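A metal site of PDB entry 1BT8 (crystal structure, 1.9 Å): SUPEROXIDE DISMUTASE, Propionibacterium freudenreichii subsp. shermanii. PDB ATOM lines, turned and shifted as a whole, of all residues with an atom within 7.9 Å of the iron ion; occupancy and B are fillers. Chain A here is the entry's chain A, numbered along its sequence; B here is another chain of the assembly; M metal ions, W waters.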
ATOM      1  N   HIS A  27     -14.208 -19.607  18.406  1.00  0.00           N
ATOM      2  CA  HIS A  27     -13.716 -20.620  19.322  1.00  0.00           C
ATOM      3  C   HIS A  27     -12.796 -21.649  18.679  1.00  0.00           C
ATOM      4  O   HIS A  27     -11.804 -22.074  19.275  1.00  0.00           O
ATOM      5  CB  HIS A  27     -14.906 -21.324  19.970  1.00  0.00           C
ATOM      6  CG  HIS A  27     -14.615 -21.905  21.314  1.00  0.00           C
ATOM      7  ND1 HIS A  27     -15.577 -22.540  22.081  1.00  0.00           N
ATOM      8  CD2 HIS A  27     -13.472 -21.948  22.044  1.00  0.00           C
ATOM      9  CE1 HIS A  27     -15.043 -22.942  23.207  1.00  0.00           C
ATOM     10  NE2 HIS A  27     -13.773 -22.602  23.218  1.00  0.00           N
ATOM     11  N   HIS A  28     -13.117 -22.055  17.456  1.00  0.00           N
ATOM     12  CA  HIS A  28     -12.340 -23.041  16.730  1.00  0.00           C
ATOM     13  C   HIS A  28     -11.230 -22.421  15.877  1.00  0.00           C
ATOM     14  O   HIS A  28     -10.050 -22.756  16.028  1.00  0.00           O
ATOM     15  CB  HIS A  28     -13.265 -23.894  15.854  1.00  0.00           C
ATOM     16  CG  HIS A  28     -12.552 -24.849  14.942  1.00  0.00           C
ATOM     17  ND1 HIS A  28     -12.290 -24.551  13.619  1.00  0.00           N
ATOM     18  CD2 HIS A  28     -12.044 -26.073  15.167  1.00  0.00           C
ATOM     19  CE1 HIS A  28     -11.640 -25.561  13.073  1.00  0.00           C
ATOM     20  NE2 HIS A  28     -11.474 -26.503  13.987  1.00  0.00           N
ATOM     21  N   HIS A  31      -9.301 -19.391  18.824  1.00  0.00           N
ATOM     22  CA  HIS A  31      -8.856 -19.971  20.081  1.00  0.00           C
ATOM     23  C   HIS A  31      -8.128 -21.303  20.006  1.00  0.00           C
ATOM     24  O   HIS A  31      -6.991 -21.416  20.481  1.00  0.00           O
ATOM     25  CB  HIS A  31     -10.021 -20.050  21.073  1.00  0.00           C
ATOM     26  CG  HIS A  31     -10.463 -18.728  21.596  1.00  0.00           C
ATOM     27  ND1 HIS A  31      -9.874 -18.121  22.694  1.00  0.00           N
ATOM     28  CD2 HIS A  31     -11.421 -17.868  21.176  1.00  0.00           C
ATOM     29  CE1 HIS A  31     -10.444 -16.958  22.918  1.00  0.00           C
ATOM     30  NE2 HIS A  31     -11.391 -16.775  22.010  1.00  0.00           N
ATOM     31  N   HIS A  32      -8.764 -22.321  19.416  1.00  0.00           N
ATOM     32  CA  HIS A  32      -8.142 -23.642  19.312  1.00  0.00           C
ATOM     33  C   HIS A  32      -6.848 -23.603  18.503  1.00  0.00           C
ATOM     34  O   HIS A  32      -5.861 -24.212  18.895  1.00  0.00           O
ATOM     35  CB  HIS A  32      -9.119 -24.656  18.722  1.00  0.00           C
ATOM     36  CG  HIS A  32      -8.741 -26.087  18.962  1.00  0.00           C
ATOM     37  ND1 HIS A  32      -9.636 -27.117  18.843  1.00  0.00           N
ATOM     38  CD2 HIS A  32      -7.567 -26.655  19.328  1.00  0.00           C
ATOM     39  CE1 HIS A  32      -9.032 -28.265  19.123  1.00  0.00           C
ATOM     40  NE2 HIS A  32      -7.768 -28.000  19.415  1.00  0.00           N
ATOM     41  N   TYR A  35      -3.744 -22.680  20.565  1.00  0.00           N
ATOM     42  CA  TYR A  35      -3.180 -23.717  21.430  1.00  0.00           C
ATOM     43  C   TYR A  35      -2.271 -24.658  20.641  1.00  0.00           C
ATOM     44  O   TYR A  35      -1.307 -25.182  21.174  1.00  0.00           O
ATOM     45  CB  TYR A  35      -4.285 -24.530  22.107  1.00  0.00           C
ATOM     46  CG  TYR A  35      -5.266 -23.702  22.907  1.00  0.00           C
ATOM     47  CD1 TYR A  35      -4.817 -22.816  23.891  1.00  0.00           C
ATOM     48  CD2 TYR A  35      -6.630 -23.799  22.675  1.00  0.00           C
ATOM     49  CE1 TYR A  35      -5.721 -22.041  24.618  1.00  0.00           C
ATOM     50  CE2 TYR A  35      -7.533 -23.036  23.398  1.00  0.00           C
ATOM     51  CZ  TYR A  35      -7.081 -22.153  24.368  1.00  0.00           C
ATOM     52  OH  TYR A  35      -7.982 -21.404  25.086  1.00  0.00           O
ATOM     53  N   GLY A  71      -5.022 -27.291  26.367  1.00  0.00           N
ATOM     54  CA  GLY A  71      -6.064 -26.569  25.662  1.00  0.00           C
ATOM     55  C   GLY A  71      -6.429 -27.332  24.401  1.00  0.00           C
ATOM     56  O   GLY A  71      -7.610 -27.484  24.079  1.00  0.00           O
ATOM     57  N   ASN A  74      -8.334 -30.534  25.505  1.00  0.00           N
ATOM     58  CA  ASN A  74      -9.666 -30.216  26.010  1.00  0.00           C
ATOM     59  C   ASN A  74     -10.668 -29.835  24.930  1.00  0.00           C
ATOM     60  O   ASN A  74     -11.826 -30.242  24.984  1.00  0.00           O
ATOM     61  CB  ASN A  74      -9.600 -29.108  27.065  1.00  0.00           C
ATOM     62  CG  ASN A  74      -8.917 -29.561  28.345  1.00  0.00           C
ATOM     63  OD1 ASN A  74      -8.599 -30.744  28.528  1.00  0.00           O
ATOM     64  ND2 ASN A  74      -8.690 -28.617  29.251  1.00  0.00           N
ATOM     65  N   HIS A  75     -10.222 -29.064  23.941  1.00  0.00           N
ATOM     66  CA  HIS A  75     -11.115 -28.654  22.861  1.00  0.00           C
ATOM     67  C   HIS A  75     -11.372 -29.765  21.846  1.00  0.00           C
ATOM     68  O   HIS A  75     -12.465 -29.848  21.294  1.00  0.00           O
ATOM     69  CB  HIS A  75     -10.591 -27.386  22.181  1.00  0.00           C
ATOM     70  CG  HIS A  75     -10.689 -26.166  23.038  1.00  0.00           C
ATOM     71  ND1 HIS A  75      -9.669 -25.768  23.880  1.00  0.00           N
ATOM     72  CD2 HIS A  75     -11.699 -25.283  23.218  1.00  0.00           C
ATOM     73  CE1 HIS A  75     -10.054 -24.692  24.541  1.00  0.00           C
ATOM     74  NE2 HIS A  75     -11.282 -24.380  24.167  1.00  0.00           N
ATOM     75  N   PHE A  78     -14.064 -31.725  23.280  1.00  0.00           N
ATOM     76  CA  PHE A  78     -15.210 -30.831  23.340  1.00  0.00           C
ATOM     77  C   PHE A  78     -16.022 -30.791  22.042  1.00  0.00           C
ATOM     78  O   PHE A  78     -17.249 -30.875  22.059  1.00  0.00           O
ATOM     79  CB  PHE A  78     -14.741 -29.419  23.712  1.00  0.00           C
ATOM     80  CG  PHE A  78     -15.854 -28.429  23.955  1.00  0.00           C
ATOM     81  CD1 PHE A  78     -16.915 -28.743  24.797  1.00  0.00           C
ATOM     82  CD2 PHE A  78     -15.825 -27.173  23.357  1.00  0.00           C
ATOM     83  CE1 PHE A  78     -17.932 -27.826  25.050  1.00  0.00           C
ATOM     84  CE2 PHE A  78     -16.832 -26.242  23.595  1.00  0.00           C
ATOM     85  CZ  PHE A  78     -17.895 -26.567  24.446  1.00  0.00           C
ATOM     86  N   TRP A  79     -15.332 -30.668  20.910  1.00  0.00           N
ATOM     87  CA  TRP A  79     -15.993 -30.624  19.606  1.00  0.00           C
ATOM     88  C   TRP A  79     -16.770 -31.908  19.330  1.00  0.00           C
ATOM     89  O   TRP A  79     -17.953 -31.862  19.020  1.00  0.00           O
ATOM     90  CB  TRP A  79     -14.973 -30.411  18.483  1.00  0.00           C
ATOM     91  CG  TRP A  79     -14.114 -29.166  18.580  1.00  0.00           C
ATOM     92  CD1 TRP A  79     -12.797 -29.060  18.232  1.00  0.00           C
ATOM     93  CD2 TRP A  79     -14.523 -27.852  19.024  1.00  0.00           C
ATOM     94  NE1 TRP A  79     -12.365 -27.778  18.434  1.00  0.00           N
ATOM     95  CE2 TRP A  79     -13.397 -27.018  18.922  1.00  0.00           C
ATOM     96  CE3 TRP A  79     -15.726 -27.321  19.499  1.00  0.00           C
ATOM     97  CZ2 TRP A  79     -13.433 -25.659  19.276  1.00  0.00           C
ATOM     98  CZ3 TRP A  79     -15.762 -25.963  19.853  1.00  0.00           C
ATOM     99  CH2 TRP A  79     -14.627 -25.152  19.736  1.00  0.00           C
ATOM    100  N   GLY A 125     -12.108 -22.428  33.520  1.00  0.00           N
ATOM    101  CA  GLY A 125     -12.025 -23.856  33.787  1.00  0.00           C
ATOM    102  C   GLY A 125     -12.979 -24.746  32.993  1.00  0.00           C
ATOM    103  O   GLY A 125     -13.605 -24.303  32.035  1.00  0.00           O
ATOM    104  N   TRP A 126     -13.055 -26.010  33.409  1.00  0.00           N
ATOM    105  CA  TRP A 126     -13.906 -27.009  32.752  1.00  0.00           C
ATOM    106  C   TRP A 126     -14.608 -27.921  33.739  1.00  0.00           C
ATOM    107  O   TRP A 126     -14.151 -28.126  34.866  1.00  0.00           O
ATOM    108  CB  TRP A 126     -13.063 -27.931  31.852  1.00  0.00           C
ATOM    109  CG  TRP A 126     -12.304 -27.247  30.777  1.00  0.00           C
ATOM    110  CD1 TRP A 126     -11.235 -26.429  30.931  1.00  0.00           C
ATOM    111  CD2 TRP A 126     -12.551 -27.322  29.365  1.00  0.00           C
ATOM    112  NE1 TRP A 126     -10.803 -25.969  29.710  1.00  0.00           N
ATOM    113  CE2 TRP A 126     -11.600 -26.501  28.729  1.00  0.00           C
ATOM    114  CE3 TRP A 126     -13.501 -27.999  28.582  1.00  0.00           C
ATOM    115  CZ2 TRP A 126     -11.552 -26.342  27.341  1.00  0.00           C
ATOM    116  CZ3 TRP A 126     -13.449 -27.835  27.202  1.00  0.00           C
ATOM    117  CH2 TRP A 126     -12.488 -27.009  26.597  1.00  0.00           C
ATOM    118  N   HIS A 146      -6.900 -24.819  31.987  1.00  0.00           N
ATOM    119  CA  HIS A 146      -6.919 -25.984  31.104  1.00  0.00           C
ATOM    120  C   HIS A 146      -6.162 -27.171  31.700  1.00  0.00           C
ATOM    121  O   HIS A 146      -6.512 -28.327  31.473  1.00  0.00           O
ATOM    122  CB  HIS A 146      -6.250 -25.669  29.758  1.00  0.00           C
ATOM    123  CG  HIS A 146      -7.058 -24.787  28.867  1.00  0.00           C
ATOM    124  ND1 HIS A 146      -6.510 -23.705  28.208  1.00  0.00           N
ATOM    125  CD2 HIS A 146      -8.355 -24.842  28.503  1.00  0.00           C
ATOM    126  CE1 HIS A 146      -7.449 -23.125  27.477  1.00  0.00           C
ATOM    127  NE2 HIS A 146      -8.572 -23.792  27.636  1.00  0.00           N
ATOM    128  N   LEU A 160     -16.984 -29.847  29.230  1.00  0.00           N
ATOM    129  CA  LEU A 160     -17.739 -28.610  29.012  1.00  0.00           C
ATOM    130  C   LEU A 160     -16.831 -27.414  29.303  1.00  0.00           C
ATOM    131  O   LEU A 160     -16.321 -27.264  30.410  1.00  0.00           O
ATOM    132  CB  LEU A 160     -18.972 -28.566  29.917  1.00  0.00           C
ATOM    133  CG  LEU A 160     -19.785 -27.268  29.970  1.00  0.00           C
ATOM    134  CD1 LEU A 160     -20.210 -26.835  28.575  1.00  0.00           C
ATOM    135  CD2 LEU A 160     -20.996 -27.463  30.853  1.00  0.00           C
ATOM    136  N   ASP A 161     -16.613 -26.585  28.280  1.00  0.00           N
ATOM    137  CA  ASP A 161     -15.763 -25.409  28.403  1.00  0.00           C
ATOM    138  C   ASP A 161     -16.472 -24.303  29.183  1.00  0.00           C
ATOM    139  O   ASP A 161     -17.485 -23.770  28.724  1.00  0.00           O
ATOM    140  CB  ASP A 161     -15.371 -24.890  27.004  1.00  0.00           C
ATOM    141  CG  ASP A 161     -14.249 -23.853  27.032  1.00  0.00           C
ATOM    142  OD1 ASP A 161     -13.787 -23.469  28.125  1.00  0.00           O
ATOM    143  OD2 ASP A 161     -13.806 -23.437  25.942  1.00  0.00           O
ATOM    144  N   MET A 162     -15.946 -23.983  30.365  1.00  0.00           N
ATOM    145  CA  MET A 162     -16.557 -22.942  31.175  1.00  0.00           C
ATOM    146  C   MET A 162     -15.824 -21.604  31.131  1.00  0.00           C
ATOM    147  O   MET A 162     -16.092 -20.712  31.934  1.00  0.00           O
ATOM    148  CB  MET A 162     -16.757 -23.415  32.623  1.00  0.00           C
ATOM    149  CG  MET A 162     -17.881 -24.434  32.784  1.00  0.00           C
ATOM    150  SD  MET A 162     -19.433 -23.921  32.011  1.00  0.00           S
ATOM    151  CE  MET A 162     -20.004 -22.638  33.126  1.00  0.00           C
ATOM    152  N   TRP A 163     -14.895 -21.469  30.179  1.00  0.00           N
ATOM    153  CA  TRP A 163     -14.182 -20.190  30.000  1.00  0.00           C
ATOM    154  C   TRP A 163     -15.230 -19.232  29.456  1.00  0.00           C
ATOM    155  O   TRP A 163     -16.136 -19.646  28.721  1.00  0.00           O
ATOM    156  CB  TRP A 163     -13.045 -20.340  28.994  1.00  0.00           C
ATOM    157  CG  TRP A 163     -11.798 -20.975  29.527  1.00  0.00           C
ATOM    158  CD1 TRP A 163     -11.698 -22.177  30.162  1.00  0.00           C
ATOM    159  CD2 TRP A 163     -10.467 -20.457  29.422  1.00  0.00           C
ATOM    160  NE1 TRP A 163     -10.375 -22.449  30.457  1.00  0.00           N
ATOM    161  CE2 TRP A 163      -9.597 -21.410  30.008  1.00  0.00           C
ATOM    162  CE3 TRP A 163      -9.919 -19.282  28.886  1.00  0.00           C
ATOM    163  CZ2 TRP A 163      -8.222 -21.219  30.075  1.00  0.00           C
ATOM    164  CZ3 TRP A 163      -8.542 -19.104  28.949  1.00  0.00           C
ATOM    165  CH2 TRP A 163      -7.705 -20.062  29.542  1.00  0.00           C
ATOM    166  N   GLU A 164     -15.094 -17.951  29.781  1.00  0.00           N
ATOM    167  CA  GLU A 164     -16.065 -16.948  29.337  1.00  0.00           C
ATOM    168  C   GLU A 164     -16.267 -16.786  27.831  1.00  0.00           C
ATOM    169  O   GLU A 164     -17.362 -16.455  27.384  1.00  0.00           O
ATOM    170  CB  GLU A 164     -15.775 -15.591  29.992  1.00  0.00           C
ATOM    171  CG  GLU A 164     -15.926 -15.644  31.511  1.00  0.00           C
ATOM    172  CD  GLU A 164     -15.619 -14.331  32.187  1.00  0.00           C
ATOM    173  OE1 GLU A 164     -14.603 -13.696  31.843  1.00  0.00           O
ATOM    174  OE2 GLU A 164     -16.406 -13.927  33.078  1.00  0.00           O
ATOM    175  N   HIS A 165     -15.227 -17.052  27.039  1.00  0.00           N
ATOM    176  CA  HIS A 165     -15.319 -16.939  25.587  1.00  0.00           C
ATOM    177  C   HIS A 165     -16.270 -17.978  24.986  1.00  0.00           C
ATOM    178  O   HIS A 165     -16.743 -17.830  23.866  1.00  0.00           O
ATOM    179  CB  HIS A 165     -13.941 -17.062  24.936  1.00  0.00           C
ATOM    180  CG  HIS A 165     -13.257 -18.366  25.186  1.00  0.00           C
ATOM    181  ND1 HIS A 165     -12.086 -18.466  25.913  1.00  0.00           N
ATOM    182  CD2 HIS A 165     -13.548 -19.626  24.772  1.00  0.00           C
ATOM    183  CE1 HIS A 165     -11.689 -19.728  25.946  1.00  0.00           C
ATOM    184  NE2 HIS A 165     -12.564 -20.448  25.258  1.00  0.00           N
ATOM    185  N   ALA A 166     -16.535 -19.036  25.751  1.00  0.00           N
ATOM    186  CA  ALA A 166     -17.408 -20.108  25.304  1.00  0.00           C
ATOM    187  C   ALA A 166     -18.909 -19.797  25.387  1.00  0.00           C
ATOM    188  O   ALA A 166     -19.713 -20.515  24.792  1.00  0.00           O
ATOM    189  CB  ALA A 166     -17.110 -21.385  26.081  1.00  0.00           C
ATOM    190  N   TYR A 178     -26.457 -21.280  29.859  1.00  0.00           N
ATOM    191  CA  TYR A 178     -25.504 -21.898  28.943  1.00  0.00           C
ATOM    192  C   TYR A 178     -25.413 -23.416  29.147  1.00  0.00           C
ATOM    193  O   TYR A 178     -25.522 -24.177  28.183  1.00  0.00           O
ATOM    194  CB  TYR A 178     -24.123 -21.256  29.138  1.00  0.00           C
ATOM    195  CG  TYR A 178     -22.968 -21.990  28.483  1.00  0.00           C
ATOM    196  CD1 TYR A 178     -22.924 -22.195  27.107  1.00  0.00           C
ATOM    197  CD2 TYR A 178     -21.897 -22.453  29.248  1.00  0.00           C
ATOM    198  CE1 TYR A 178     -21.839 -22.844  26.499  1.00  0.00           C
ATOM    199  CE2 TYR A 178     -20.806 -23.103  28.664  1.00  0.00           C
ATOM    200  CZ  TYR A 178     -20.788 -23.296  27.294  1.00  0.00           C
ATOM    201  OH  TYR A 178     -19.712 -23.921  26.701  1.00  0.00           O
ATOM    202  N   GLU B 164     -11.939 -12.158  30.261  1.00  0.00           N
ATOM    203  CA  GLU B 164     -12.675 -12.059  29.001  1.00  0.00           C
ATOM    204  C   GLU B 164     -13.969 -11.243  29.023  1.00  0.00           C
ATOM    205  O   GLU B 164     -14.277 -10.566  28.050  1.00  0.00           O
ATOM    206  CB  GLU B 164     -12.913 -13.445  28.417  1.00  0.00           C
ATOM    207  CG  GLU B 164     -11.621 -14.115  27.949  1.00  0.00           C
ATOM    208  CD  GLU B 164     -11.782 -15.563  27.538  1.00  0.00           C
ATOM    209  OE1 GLU B 164     -12.647 -16.269  28.114  1.00  0.00           O
ATOM    210  OE2 GLU B 164     -11.028 -16.009  26.655  1.00  0.00           O
HETATM  211 FE    FE M   1     -12.437 -22.655  24.968  1.00  0.00          FE
HETATM  212  O   HOH W   1     -10.766 -21.832  23.879  1.00  0.00           O
HETATM  213  O   HOH W   2     -11.162 -22.916  26.788  1.00  0.00           O
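Water W2 bridges a ring nitrogen (NE2) of His 146 and the side-chain carboxylate (OD1) of Asp 161.
The iron ion is bound by the side-chain carboxylate of Asp 161 (1.9 Å), water W1 (2.2 Å), a ring nitrogen (NE2) of His 27 (2.2 Å), a ring nitrogen (NE2) of His 75 (2.2 Å), a ring nitrogen (NE2) of His 165 (2.2 Å) and water W2 (2.2 Å).
The iron ion has six donor atoms within binding distance.
The backbone carbonyl oxygen of Asp 161 sits at hydrogen-bond distance from the side-chain hydroxyl of Tyr 178.
A ring nitrogen (ND1) of His 165 lies within hydrogen-bond range of the side-chain carboxylate of Glu 164 of chain B (2.8 Å).
The backbone carbonyl oxygen of His 27 is in hydrogen-bond range of the backbone NH of His 32 (3.1 Å).
ND1 of His 75 lies within hydrogen-bond range of O of Gly 71 (2.7 Å).
The side-chain carboxylate (OD1) of Asp 161 is in hydrogen-bond range of the backbone NH (N) of Trp 163 (3.1 Å).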
